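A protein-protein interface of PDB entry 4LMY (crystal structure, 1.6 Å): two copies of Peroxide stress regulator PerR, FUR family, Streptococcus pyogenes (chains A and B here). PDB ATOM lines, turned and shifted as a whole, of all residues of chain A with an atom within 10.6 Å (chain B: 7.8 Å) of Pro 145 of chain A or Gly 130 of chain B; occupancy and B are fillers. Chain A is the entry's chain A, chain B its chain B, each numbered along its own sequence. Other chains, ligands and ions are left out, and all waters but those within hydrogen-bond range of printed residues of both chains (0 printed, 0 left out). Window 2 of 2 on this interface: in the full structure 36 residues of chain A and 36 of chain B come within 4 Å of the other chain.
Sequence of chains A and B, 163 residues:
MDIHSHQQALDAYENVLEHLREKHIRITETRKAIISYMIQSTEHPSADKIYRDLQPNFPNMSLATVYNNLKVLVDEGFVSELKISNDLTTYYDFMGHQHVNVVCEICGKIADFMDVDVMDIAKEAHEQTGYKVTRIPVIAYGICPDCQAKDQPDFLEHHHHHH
O of Gly 130 of chain B sits close to OE1 of Gln 148 of chain A (2.9 Å).
The backbone NH (N) of Lys 132 of chain B is in hydrogen-bond range of the side-chain amide oxygen (OE1) of Gln 148 of chain A (3.5 Å).
The backbone NH (N) of Ile 143 of chain A lies within hydrogen-bond range of the backbone carbonyl oxygen (O) of Lys 132 of chain B, at 2.9 Å.
The side-chain amide oxygen (OE1) of Gln 128 of chain B lies within hydrogen-bond range of the backbone NH (N) of Met 114 of chain A (2.8 Å).
The backbone carbonyl oxygen (O) of Lys 109 of chain A lies within hydrogen-bond range of the side-chain hydroxyl (OH) of Tyr 131 of chain B, at 2.8 Å.
O of Gly 142 of chain A is in hydrogen-bond range of N of Glu 105 of chain A, at 2.8 Å.
The side-chain sulfur (SG) of Cys 107 of chain A sits close to the side-chain amino group (NZ) of Lys 109 of chain A (3.0 Å).
The backbone NH (N) of Gly 142 of chain A lies within hydrogen-bond range of the backbone carbonyl oxygen (O) of Val 103 of chain A, at 3.0 Å.
The backbone NH (N) of Ile 106 of chain A lies close to the side-chain sulfur (SG) of Cys 104 of chain A (3.5 Å).
O of Tyr 131 of chain B sits at hydrogen-bond distance from ND1 of His 126 of chain B.
N of Val 102 of chain A is in hydrogen-bond range of O of Ala 111 of chain A (2.6 Å).
Among the printed residues, pairs that only touch across the chains: Ile 3 of chain A with Gln 128 of chain B (3.4 Å), Val 102 of chain A with Tyr 131 of chain B (3.5 Å), Val 103 of chain A with Tyr 131 of chain B (3.9 Å), Cys 104 of chain A with Tyr 131 of chain B (3.6 Å), Ile 110 of chain A with Tyr 131 of chain B (3.8 Å), Ala 111 of chain A with Thr 129 of chain B (3.9 Å), Ala 111 of chain A with Tyr 131 of chain B (3.6 Å), Asp 112 of chain A with Thr 129 of chain B (3.7 Å), Phe 113 of chain A with Ala 125 of chain B (3.6 Å), Phe 113 of chain A with Gln 128 of chain B (3.5 Å), Tyr 141 of chain A with Val 133 of chain B (3.5 Å), Gly 142 of chain A with Lys 132 of chain B (3.1 Å), Gly 142 of chain A with Val 133 of chain B (3.99 Å), Ile 143 of chain A with Tyr 131 of chain B (3.3 Å), Cys 144 of chain A with Tyr 131 of chain B (3.4 Å), Pro 145 of chain A with Thr 129 of chain B (3.8 Å), Pro 145 of chain A with Gly 130 of chain B (3.8 Å), Pro 145 of chain A with Tyr 131 of chain B (3.8 Å) and Gln 148 of chain A with Tyr 131 of chain B (3.9 Å).
Printed residues of chain B within 4 Å of Pro 145 of chain A: Thr 129, Gly 130 and Tyr 131.
No residue of chain A comes within 4 Å of His 126 of chain B.
Thr 129 of chain B touches three residues of chain A.
Of chain A, only Val 102, Val 103, Cys 104, Lys 109, Ile 110, Ala 111, Ile 143, Cys 144, Pro 145 and Gln 148 come within 4 Å of Tyr 131 of chain B.
Of the printed residues of chain A, Gln 128 of chain B touches Ile 3 (3.4 Å), Phe 113 (3.5 Å) and Met 114 (2.8 Å).
Of the printed residues of chain B, Val 102 of chain A touches Tyr 131.
Printed residues of chain B within 4 Å of Ile 3 of chain A: Gln 128 (3.4 Å).
Printed residues of chain B within 4 Å of Lys 109 of chain A: Tyr 131.
The nearest residue of chain B that does not touch Pro 145 of chain A is Lys 132 of chain B (5.9 Å).
Of the 11 printed residues of chain B, 7 touch a printed residue of chain A.
Along chain B the printed residues that touch a printed residue of chain A span positions 125 to 133.
Hydrophobic or aromatic side chains of chain A within 4 Å of the printed part of chain B: Ile 3, Val 102, Ala 111, Phe 113, Met 114 and Pro 145.
Along chain A the printed residues that touch a printed residue of chain B span positions 3 to 148.
Among the printed residues, no Asp or Glu carboxylate lies within 4 Å of a Lys or Arg side-chain nitrogen of the other chain.
No position is printed for both chains.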
ATOM      1  N   ILE A   3     -31.832 -18.984  31.723  1.00  0.00           N
ATOM      2  CA  ILE A   3     -31.416 -19.348  30.375  1.00  0.00           C
ATOM      3  C   ILE A   3     -30.381 -20.475  30.426  1.00  0.00           C
ATOM      4  O   ILE A   3     -29.447 -20.446  31.227  1.00  0.00           O
ATOM      5  CB  ILE A   3     -30.873 -18.120  29.603  1.00  0.00           C
ATOM      6  CG1 ILE A   3     -32.012 -17.139  29.315  1.00  0.00           C
ATOM      7  CG2 ILE A   3     -30.211 -18.543  28.303  1.00  0.00           C
ATOM      8  CD1 ILE A   3     -31.597 -15.928  28.505  1.00  0.00           C
ATOM      9  N   VAL A 102     -31.056 -22.288  15.726  1.00  0.00           N
ATOM     10  CA  VAL A 102     -30.762 -21.237  14.764  1.00  0.00           C
ATOM     11  C   VAL A 102     -29.692 -21.778  13.825  1.00  0.00           C
ATOM     12  O   VAL A 102     -28.644 -22.245  14.273  1.00  0.00           O
ATOM     13  CB  VAL A 102     -30.238 -19.952  15.431  1.00  0.00           C
ATOM     14  CG1 VAL A 102     -30.264 -18.798  14.438  1.00  0.00           C
ATOM     15  CG2 VAL A 102     -31.063 -19.613  16.650  1.00  0.00           C
ATOM     16  N   VAL A 103     -29.972 -21.731  12.529  1.00  0.00           N
ATOM     17  CA  VAL A 103     -29.070 -22.298  11.532  1.00  0.00           C
ATOM     18  C   VAL A 103     -28.374 -21.198  10.737  1.00  0.00           C
ATOM     19  O   VAL A 103     -29.020 -20.275  10.251  1.00  0.00           O
ATOM     20  CB  VAL A 103     -29.836 -23.221  10.559  1.00  0.00           C
ATOM     21  CG1 VAL A 103     -28.890 -23.811   9.526  1.00  0.00           C
ATOM     22  CG2 VAL A 103     -30.549 -24.325  11.322  1.00  0.00           C
ATOM     23  N   CYS A 104     -27.052 -21.289  10.605  1.00  0.00           N
ATOM     24  CA  CYS A 104     -26.336 -20.302   9.809  1.00  0.00           C
ATOM     25  C   CYS A 104     -26.622 -20.508   8.326  1.00  0.00           C
ATOM     26  O   CYS A 104     -26.465 -21.610   7.800  1.00  0.00           O
ATOM     27  CB  CYS A 104     -24.829 -20.351  10.067  1.00  0.00           C
ATOM     28  SG  CYS A 104     -23.920 -19.038   9.211  1.00  0.00           S
ATOM     29  N   GLU A 105     -27.047 -19.438   7.663  1.00  0.00           N
ATOM     30  CA  GLU A 105     -27.359 -19.475   6.237  1.00  0.00           C
ATOM     31  C   GLU A 105     -26.117 -19.785   5.410  1.00  0.00           C
ATOM     32  O   GLU A 105     -26.203 -20.390   4.339  1.00  0.00           O
ATOM     33  CB  GLU A 105     -27.940 -18.131   5.794  1.00  0.00           C
ATOM     34  CG  GLU A 105     -29.179 -17.697   6.562  1.00  0.00           C
ATOM     35  CD  GLU A 105     -30.466 -17.966   5.804  1.00  0.00           C
ATOM     36  OE1 GLU A 105     -31.409 -17.160   5.940  1.00  0.00           O
ATOM     37  OE2 GLU A 105     -30.537 -18.977   5.073  1.00  0.00           O
ATOM     38  N   ILE A 106     -24.962 -19.366   5.913  1.00  0.00           N
ATOM     39  CA  ILE A 106     -23.717 -19.503   5.164  1.00  0.00           C
ATOM     40  C   ILE A 106     -23.020 -20.843   5.397  1.00  0.00           C
ATOM     41  O   ILE A 106     -22.798 -21.601   4.453  1.00  0.00           O
ATOM     42  CB  ILE A 106     -22.753 -18.339   5.463  1.00  0.00           C
ATOM     43  CG1 ILE A 106     -23.410 -17.008   5.081  1.00  0.00           C
ATOM     44  CG2 ILE A 106     -21.439 -18.531   4.716  1.00  0.00           C
ATOM     45  CD1 ILE A 106     -22.540 -15.789   5.310  1.00  0.00           C
ATOM     46  N   CYS A 107     -22.681 -21.140   6.646  1.00  0.00           N
ATOM     47  CA  CYS A 107     -21.905 -22.344   6.941  1.00  0.00           C
ATOM     48  C   CYS A 107     -22.745 -23.525   7.425  1.00  0.00           C
ATOM     49  O   CYS A 107     -22.299 -24.668   7.365  1.00  0.00           O
ATOM     50  CB  CYS A 107     -20.787 -22.045   7.940  1.00  0.00           C
ATOM     51  SG  CYS A 107     -21.363 -21.784   9.636  1.00  0.00           S
ATOM     52  N   GLY A 108     -23.954 -23.254   7.909  1.00  0.00           N
ATOM     53  CA  GLY A 108     -24.845 -24.317   8.334  1.00  0.00           C
ATOM     54  C   GLY A 108     -24.683 -24.749   9.780  1.00  0.00           C
ATOM     55  O   GLY A 108     -25.393 -25.637  10.246  1.00  0.00           O
ATOM     56  N   LYS A 109     -23.754 -24.122  10.496  1.00  0.00           N
ATOM     57  CA  LYS A 109     -23.565 -24.453  11.902  1.00  0.00           C
ATOM     58  C   LYS A 109     -24.818 -24.095  12.691  1.00  0.00           C
ATOM     59  O   LYS A 109     -25.459 -23.072  12.438  1.00  0.00           O
ATOM     60  CB  LYS A 109     -22.335 -23.749  12.480  1.00  0.00           C
ATOM     61  CG  LYS A 109     -21.017 -24.291  11.944  1.00  0.00           C
ATOM     62  CD  LYS A 109     -19.826 -23.580  12.565  1.00  0.00           C
ATOM     63  CE  LYS A 109     -18.821 -23.088  11.523  1.00  0.00           C
ATOM     64  NZ  LYS A 109     -18.887 -21.614  11.320  1.00  0.00           N
ATOM     65  N   ILE A 110     -25.168 -24.959  13.635  1.00  0.00           N
ATOM     66  CA  ILE A 110     -26.400 -24.808  14.395  1.00  0.00           C
ATOM     67  C   ILE A 110     -26.129 -24.412  15.840  1.00  0.00           C
ATOM     68  O   ILE A 110     -25.276 -24.995  16.510  1.00  0.00           O
ATOM     69  CB  ILE A 110     -27.220 -26.110  14.370  1.00  0.00           C
ATOM     70  CG1 ILE A 110     -27.577 -26.484  12.929  1.00  0.00           C
ATOM     71  CG2 ILE A 110     -28.484 -25.971  15.207  1.00  0.00           C
ATOM     72  CD1 ILE A 110     -28.253 -27.830  12.802  1.00  0.00           C
ATOM     73  N   ALA A 111     -26.853 -23.398  16.300  1.00  0.00           N
ATOM     74  CA  ALA A 111     -26.906 -23.055  17.712  1.00  0.00           C
ATOM     75  C   ALA A 111     -28.355 -23.201  18.159  1.00  0.00           C
ATOM     76  O   ALA A 111     -29.249 -23.363  17.331  1.00  0.00           O
ATOM     77  CB  ALA A 111     -26.422 -21.632  17.934  1.00  0.00           C
ATOM     78  N   ASP A 112     -28.586 -23.173  19.464  1.00  0.00           N
ATOM     79  CA  ASP A 112     -29.954 -23.198  19.965  1.00  0.00           C
ATOM     80  C   ASP A 112     -30.157 -22.141  21.035  1.00  0.00           C
ATOM     81  O   ASP A 112     -29.200 -21.683  21.663  1.00  0.00           O
ATOM     82  CB  ASP A 112     -30.339 -24.584  20.487  1.00  0.00           C
ATOM     83  CG  ASP A 112     -29.459 -25.049  21.627  1.00  0.00           C
ATOM     84  OD1 ASP A 112     -29.688 -24.616  22.780  1.00  0.00           O
ATOM     85  OD2 ASP A 112     -28.546 -25.862  21.375  1.00  0.00           O
ATOM     86  N   PHE A 113     -31.410 -21.746  21.226  1.00  0.00           N
ATOM     87  CA  PHE A 113     -31.747 -20.764  22.248  1.00  0.00           C
ATOM     88  C   PHE A 113     -33.030 -21.160  22.965  1.00  0.00           C
ATOM     89  O   PHE A 113     -33.834 -21.930  22.444  1.00  0.00           O
ATOM     90  CB  PHE A 113     -31.881 -19.364  21.643  1.00  0.00           C
ATOM     91  CG  PHE A 113     -33.058 -19.204  20.723  1.00  0.00           C
ATOM     92  CD1 PHE A 113     -34.209 -18.558  21.146  1.00  0.00           C
ATOM     93  CD2 PHE A 113     -33.012 -19.696  19.432  1.00  0.00           C
ATOM     94  CE1 PHE A 113     -35.288 -18.412  20.297  1.00  0.00           C
ATOM     95  CE2 PHE A 113     -34.087 -19.551  18.580  1.00  0.00           C
ATOM     96  CZ  PHE A 113     -35.224 -18.912  19.011  1.00  0.00           C
ATOM     97  N   MET A 114     -33.207 -20.630  24.169  1.00  0.00           N
ATOM     98  CA  MET A 114     -34.405 -20.899  24.953  1.00  0.00           C
ATOM     99  C   MET A 114     -35.542 -19.965  24.599  1.00  0.00           C
ATOM    100  O   MET A 114     -35.402 -18.742  24.653  1.00  0.00           O
ATOM    101  CB  MET A 114     -34.108 -20.755  26.434  1.00  0.00           C
ATOM    102  CG  MET A 114     -35.342 -20.847  27.321  1.00  0.00           C
ATOM    103  SD  MET A 114     -34.788 -21.038  29.012  1.00  0.00           S
ATOM    104  CE  MET A 114     -33.370 -22.026  28.656  1.00  0.00           C
ATOM    105  N   TYR A 141     -33.150 -18.863  11.245  1.00  0.00           N
ATOM    106  CA  TYR A 141     -31.975 -18.769  10.386  1.00  0.00           C
ATOM    107  C   TYR A 141     -31.269 -17.430  10.571  1.00  0.00           C
ATOM    108  O   TYR A 141     -31.900 -16.407  10.841  1.00  0.00           O
ATOM    109  CB  TYR A 141     -32.353 -18.975   8.916  1.00  0.00           C
ATOM    110  CG  TYR A 141     -32.924 -20.345   8.626  1.00  0.00           C
ATOM    111  CD1 TYR A 141     -32.102 -21.393   8.226  1.00  0.00           C
ATOM    112  CD2 TYR A 141     -34.286 -20.597   8.759  1.00  0.00           C
ATOM    113  CE1 TYR A 141     -32.621 -22.649   7.964  1.00  0.00           C
ATOM    114  CE2 TYR A 141     -34.811 -21.850   8.500  1.00  0.00           C
ATOM    115  CZ  TYR A 141     -33.975 -22.871   8.103  1.00  0.00           C
ATOM    116  OH  TYR A 141     -34.495 -24.120   7.845  1.00  0.00           O
ATOM    117  N   GLY A 142     -29.950 -17.435  10.431  1.00  0.00           N
ATOM    118  CA  GLY A 142     -29.199 -16.207  10.549  1.00  0.00           C
ATOM    119  C   GLY A 142     -27.766 -16.378  10.110  1.00  0.00           C
ATOM    120  O   GLY A 142     -27.426 -17.364   9.461  1.00  0.00           O
ATOM    121  N   ILE A 143     -26.933 -15.409  10.464  1.00  0.00           N
ATOM    122  CA  ILE A 143     -25.509 -15.476  10.179  1.00  0.00           C
ATOM    123  C   ILE A 143     -24.775 -15.637  11.500  1.00  0.00           C
ATOM    124  O   ILE A 143     -24.889 -14.788  12.383  1.00  0.00           O
ATOM    125  CB  ILE A 143     -25.009 -14.195   9.485  1.00  0.00           C
ATOM    126  CG1 ILE A 143     -25.906 -13.829   8.298  1.00  0.00           C
ATOM    127  CG2 ILE A 143     -23.566 -14.366   9.034  1.00  0.00           C
ATOM    128  CD1 ILE A 143     -25.926 -14.865   7.201  1.00  0.00           C
ATOM    129  N   CYS A 144     -24.033 -16.728  11.641  1.00  0.00           N
ATOM    130  CA  CYS A 144     -23.326 -17.007  12.890  1.00  0.00           C
ATOM    131  C   CYS A 144     -22.176 -16.018  13.098  1.00  0.00           C
ATOM    132  O   CYS A 144     -21.722 -15.388  12.147  1.00  0.00           O
ATOM    133  CB  CYS A 144     -22.811 -18.451  12.909  1.00  0.00           C
ATOM    134  SG  CYS A 144     -21.256 -18.709  11.988  1.00  0.00           S
ATOM    135  N   PRO A 145     -21.724 -15.854  14.352  1.00  0.00           N
ATOM    136  CA  PRO A 145     -20.656 -14.894  14.653  1.00  0.00           C
ATOM    137  C   PRO A 145     -19.412 -15.049  13.774  1.00  0.00           C
ATOM    138  O   PRO A 145     -18.801 -14.044  13.412  1.00  0.00           O
ATOM    139  CB  PRO A 145     -20.322 -15.205  16.110  1.00  0.00           C
ATOM    140  CG  PRO A 145     -21.622 -15.653  16.681  1.00  0.00           C
ATOM    141  CD  PRO A 145     -22.313 -16.418  15.581  1.00  0.00           C
ATOM    142  N   ASP A 146     -19.056 -16.281  13.427  1.00  0.00           N
ATOM    143  CA  ASP A 146     -17.877 -16.521  12.599  1.00  0.00           C
ATOM    144  C   ASP A 146     -18.062 -16.009  11.174  1.00  0.00           C
ATOM    145  O   ASP A 146     -17.129 -15.471  10.578  1.00  0.00           O
ATOM    146  CB  ASP A 146     -17.525 -18.010  12.572  1.00  0.00           C
ATOM    147  CG  ASP A 146     -16.760 -18.453  13.803  1.00  0.00           C
ATOM    148  OD1 ASP A 146     -16.133 -17.595  14.457  1.00  0.00           O
ATOM    149  OD2 ASP A 146     -16.778 -19.663  14.107  1.00  0.00           O
ATOM    150  N   CYS A 147     -19.266 -16.171  10.636  1.00  0.00           N
ATOM    151  CA  CYS A 147     -19.542 -15.794   9.251  1.00  0.00           C
ATOM    152  C   CYS A 147     -19.886 -14.312   9.074  1.00  0.00           C
ATOM    153  O   CYS A 147     -20.002 -13.828   7.948  1.00  0.00           O
ATOM    154  CB  CYS A 147     -20.649 -16.677   8.661  1.00  0.00           C
ATOM    155  SG  CYS A 147     -20.188 -18.415   8.423  1.00  0.00           S
ATOM    156  N   GLN A 148     -20.042 -13.595  10.185  1.00  0.00           N
ATOM    157  CA  GLN A 148     -20.340 -12.165  10.138  1.00  0.00           C
ATOM    158  C   GLN A 148     -19.117 -11.339   9.741  1.00  0.00           C
ATOM    159  O   GLN A 148     -18.000 -11.656  10.143  1.00  0.00           O
ATOM    160  CB  GLN A 148     -20.879 -11.684  11.489  1.00  0.00           C
ATOM    161  CG  GLN A 148     -22.284 -12.172  11.800  1.00  0.00           C
ATOM    162  CD  GLN A 148     -22.673 -11.951  13.249  1.00  0.00           C
ATOM    163  OE1 GLN A 148     -23.439 -12.728  13.820  1.00  0.00           O
ATOM    164  NE2 GLN A 148     -22.144 -10.892  13.853  1.00  0.00           N
ATOM    165  N   ALA A 149     -19.358 -10.286   8.957  1.00  0.00           N
ATOM    166  CA  ALA A 149     -18.335  -9.338   8.486  1.00  0.00           C
ATOM    167  C   ALA A 149     -16.939  -9.919   8.251  1.00  0.00           C
ATOM    168  O   ALA A 149     -16.789 -10.989   7.661  1.00  0.00           O
ATOM    169  CB  ALA A 149     -18.264  -8.121   9.410  1.00  0.00           C
ATOM    170  N   LYS B 123     -35.410 -11.656  18.648  1.00  0.00           N
ATOM    171  CA  LYS B 123     -34.587 -10.945  19.617  1.00  0.00           C
ATOM    172  C   LYS B 123     -33.862 -11.917  20.548  1.00  0.00           C
ATOM    173  O   LYS B 123     -32.655 -11.793  20.768  1.00  0.00           O
ATOM    174  CB  LYS B 123     -35.445  -9.969  20.424  1.00  0.00           C
ATOM    175  CG  LYS B 123     -34.700  -9.274  21.546  1.00  0.00           C
ATOM    176  CD  LYS B 123     -35.507  -8.114  22.110  1.00  0.00           C
ATOM    177  CE  LYS B 123     -34.788  -7.447  23.274  1.00  0.00           C
ATOM    178  NZ  LYS B 123     -35.442  -6.167  23.671  1.00  0.00           N
ATOM    179  N   GLU B 124     -34.601 -12.879  21.093  1.00  0.00           N
ATOM    180  CA  GLU B 124     -34.005 -13.885  21.968  1.00  0.00           C
ATOM    181  C   GLU B 124     -32.974 -14.741  21.245  1.00  0.00           C
ATOM    182  O   GLU B 124     -31.924 -15.071  21.808  1.00  0.00           O
ATOM    183  CB  GLU B 124     -35.080 -14.774  22.595  1.00  0.00           C
ATOM    184  CG  GLU B 124     -35.809 -14.123  23.753  1.00  0.00           C
ATOM    185  CD  GLU B 124     -34.878 -13.723  24.886  1.00  0.00           C
ATOM    186  OE1 GLU B 124     -33.834 -14.384  25.084  1.00  0.00           O
ATOM    187  OE2 GLU B 124     -35.195 -12.740  25.584  1.00  0.00           O
ATOM    188  N   ALA B 125     -33.282 -15.105  20.003  1.00  0.00           N
ATOM    189  CA  ALA B 125     -32.361 -15.891  19.192  1.00  0.00           C
ATOM    190  C   ALA B 125     -31.028 -15.165  19.053  1.00  0.00           C
ATOM    191  O   ALA B 125     -29.961 -15.759  19.230  1.00  0.00           O
ATOM    192  CB  ALA B 125     -32.964 -16.170  17.815  1.00  0.00           C
ATOM    193  N   HIS B 126     -31.093 -13.874  18.755  1.00  0.00           N
ATOM    194  CA  HIS B 126     -29.882 -13.075  18.614  1.00  0.00           C
ATOM    195  C   HIS B 126     -29.110 -12.978  19.924  1.00  0.00           C
ATOM    196  O   HIS B 126     -27.901 -13.191  19.956  1.00  0.00           O
ATOM    197  CB  HIS B 126     -30.215 -11.667  18.135  1.00  0.00           C
ATOM    198  CG  HIS B 126     -29.057 -10.725  18.209  1.00  0.00           C
ATOM    199  ND1 HIS B 126     -27.964 -10.824  17.375  1.00  0.00           N
ATOM    200  CD2 HIS B 126     -28.805  -9.682  19.035  1.00  0.00           C
ATOM    201  CE1 HIS B 126     -27.101  -9.869  17.668  1.00  0.00           C
ATOM    202  NE2 HIS B 126     -27.591  -9.159  18.670  1.00  0.00           N
ATOM    203  N   GLU B 127     -29.817 -12.651  21.001  1.00  0.00           N
ATOM    204  CA  GLU B 127     -29.160 -12.417  22.284  1.00  0.00           C
ATOM    205  C   GLU B 127     -28.420 -13.649  22.785  1.00  0.00           C
ATOM    206  O   GLU B 127     -27.295 -13.544  23.274  1.00  0.00           O
ATOM    207  CB  GLU B 127     -30.170 -11.944  23.333  1.00  0.00           C
ATOM    208  CG  GLU B 127     -30.735 -10.560  23.059  1.00  0.00           C
ATOM    209  CD  GLU B 127     -29.692  -9.468  23.172  1.00  0.00           C
ATOM    210  OE1 GLU B 127     -29.040  -9.368  24.233  1.00  0.00           O
ATOM    211  OE2 GLU B 127     -29.522  -8.710  22.195  1.00  0.00           O
ATOM    212  N   GLN B 128     -29.043 -14.814  22.639  1.00  0.00           N
ATOM    213  CA  GLN B 128     -28.503 -16.045  23.214  1.00  0.00           C
ATOM    214  C   GLN B 128     -27.458 -16.751  22.350  1.00  0.00           C
ATOM    215  O   GLN B 128     -26.701 -17.586  22.850  1.00  0.00           O
ATOM    216  CB  GLN B 128     -29.633 -17.021  23.548  1.00  0.00           C
ATOM    217  CG  GLN B 128     -30.594 -16.509  24.607  1.00  0.00           C
ATOM    218  CD  GLN B 128     -31.683 -17.510  24.930  1.00  0.00           C
ATOM    219  OE1 GLN B 128     -31.421 -18.702  25.088  1.00  0.00           O
ATOM    220  NE2 GLN B 128     -32.919 -17.031  25.017  1.00  0.00           N
ATOM    221  N   THR B 129     -27.419 -16.427  21.060  1.00  0.00           N
ATOM    222  CA  THR B 129     -26.529 -17.133  20.138  1.00  0.00           C
ATOM    223  C   THR B 129     -25.503 -16.223  19.473  1.00  0.00           C
ATOM    224  O   THR B 129     -24.457 -16.687  19.019  1.00  0.00           O
ATOM    225  CB  THR B 129     -27.320 -17.850  19.022  1.00  0.00           C
ATOM    226  OG1 THR B 129     -27.916 -16.877  18.154  1.00  0.00           O
ATOM    227  CG2 THR B 129     -28.399 -18.748  19.608  1.00  0.00           C
ATOM    228  N   GLY B 130     -25.804 -14.929  19.407  1.00  0.00           N
ATOM    229  CA  GLY B 130     -24.951 -13.996  18.696  1.00  0.00           C
ATOM    230  C   GLY B 130     -25.175 -13.984  17.190  1.00  0.00           C
ATOM    231  O   GLY B 130     -24.541 -13.209  16.477  1.00  0.00           O
ATOM    232  N   TYR B 131     -26.065 -14.845  16.703  1.00  0.00           N
ATOM    233  CA  TYR B 131     -26.426 -14.844  15.284  1.00  0.00           C
ATOM    234  C   TYR B 131     -27.167 -13.563  14.906  1.00  0.00           C
ATOM    235  O   TYR B 131     -27.995 -13.063  15.671  1.00  0.00           O
ATOM    236  CB  TYR B 131     -27.339 -16.027  14.946  1.00  0.00           C
ATOM    237  CG  TYR B 131     -26.671 -17.375  14.791  1.00  0.00           C
ATOM    238  CD1 TYR B 131     -26.917 -18.162  13.671  1.00  0.00           C
ATOM    239  CD2 TYR B 131     -25.811 -17.866  15.764  1.00  0.00           C
ATOM    240  CE1 TYR B 131     -26.332 -19.405  13.529  1.00  0.00           C
ATOM    241  CE2 TYR B 131     -25.216 -19.105  15.630  1.00  0.00           C
ATOM    242  CZ  TYR B 131     -25.477 -19.867  14.506  1.00  0.00           C
ATOM    243  OH  TYR B 131     -24.891 -21.104  14.369  1.00  0.00           O
ATOM    244  N   LYS B 132     -26.875 -13.036  13.720  1.00  0.00           N
ATOM    245  CA  LYS B 132     -27.704 -11.988  13.144  1.00  0.00           C
ATOM    246  C   LYS B 132     -28.849 -12.682  12.428  1.00  0.00           C
ATOM    247  O   LYS B 132     -28.650 -13.285  11.376  1.00  0.00           O
ATOM    248  CB  LYS B 132     -26.911 -11.128  12.160  1.00  0.00           C
ATOM    249  CG  LYS B 132     -27.714  -9.986  11.566  1.00  0.00           C
ATOM    250  CD  LYS B 132     -26.840  -9.075  10.728  1.00  0.00           C
ATOM    251  CE  LYS B 132     -27.193  -7.619  10.984  1.00  0.00           C
ATOM    252  NZ  LYS B 132     -27.076  -7.279  12.432  1.00  0.00           N
ATOM    253  N   VAL B 133     -30.041 -12.614  13.013  1.00  0.00           N
ATOM    254  CA  VAL B 133     -31.191 -13.366  12.517  1.00  0.00           C
ATOM    255  C   VAL B 133     -31.694 -12.840  11.173  1.00  0.00           C
ATOM    256  O   VAL B 133     -31.912 -11.642  11.010  1.00  0.00           O
ATOM    257  CB  VAL B 133     -32.350 -13.348  13.538  1.00  0.00           C
ATOM    258  CG1 VAL B 133     -33.499 -14.215  13.051  1.00  0.00           C
ATOM    259  CG2 VAL B 133     -31.863 -13.824  14.898  1.00  0.00           C
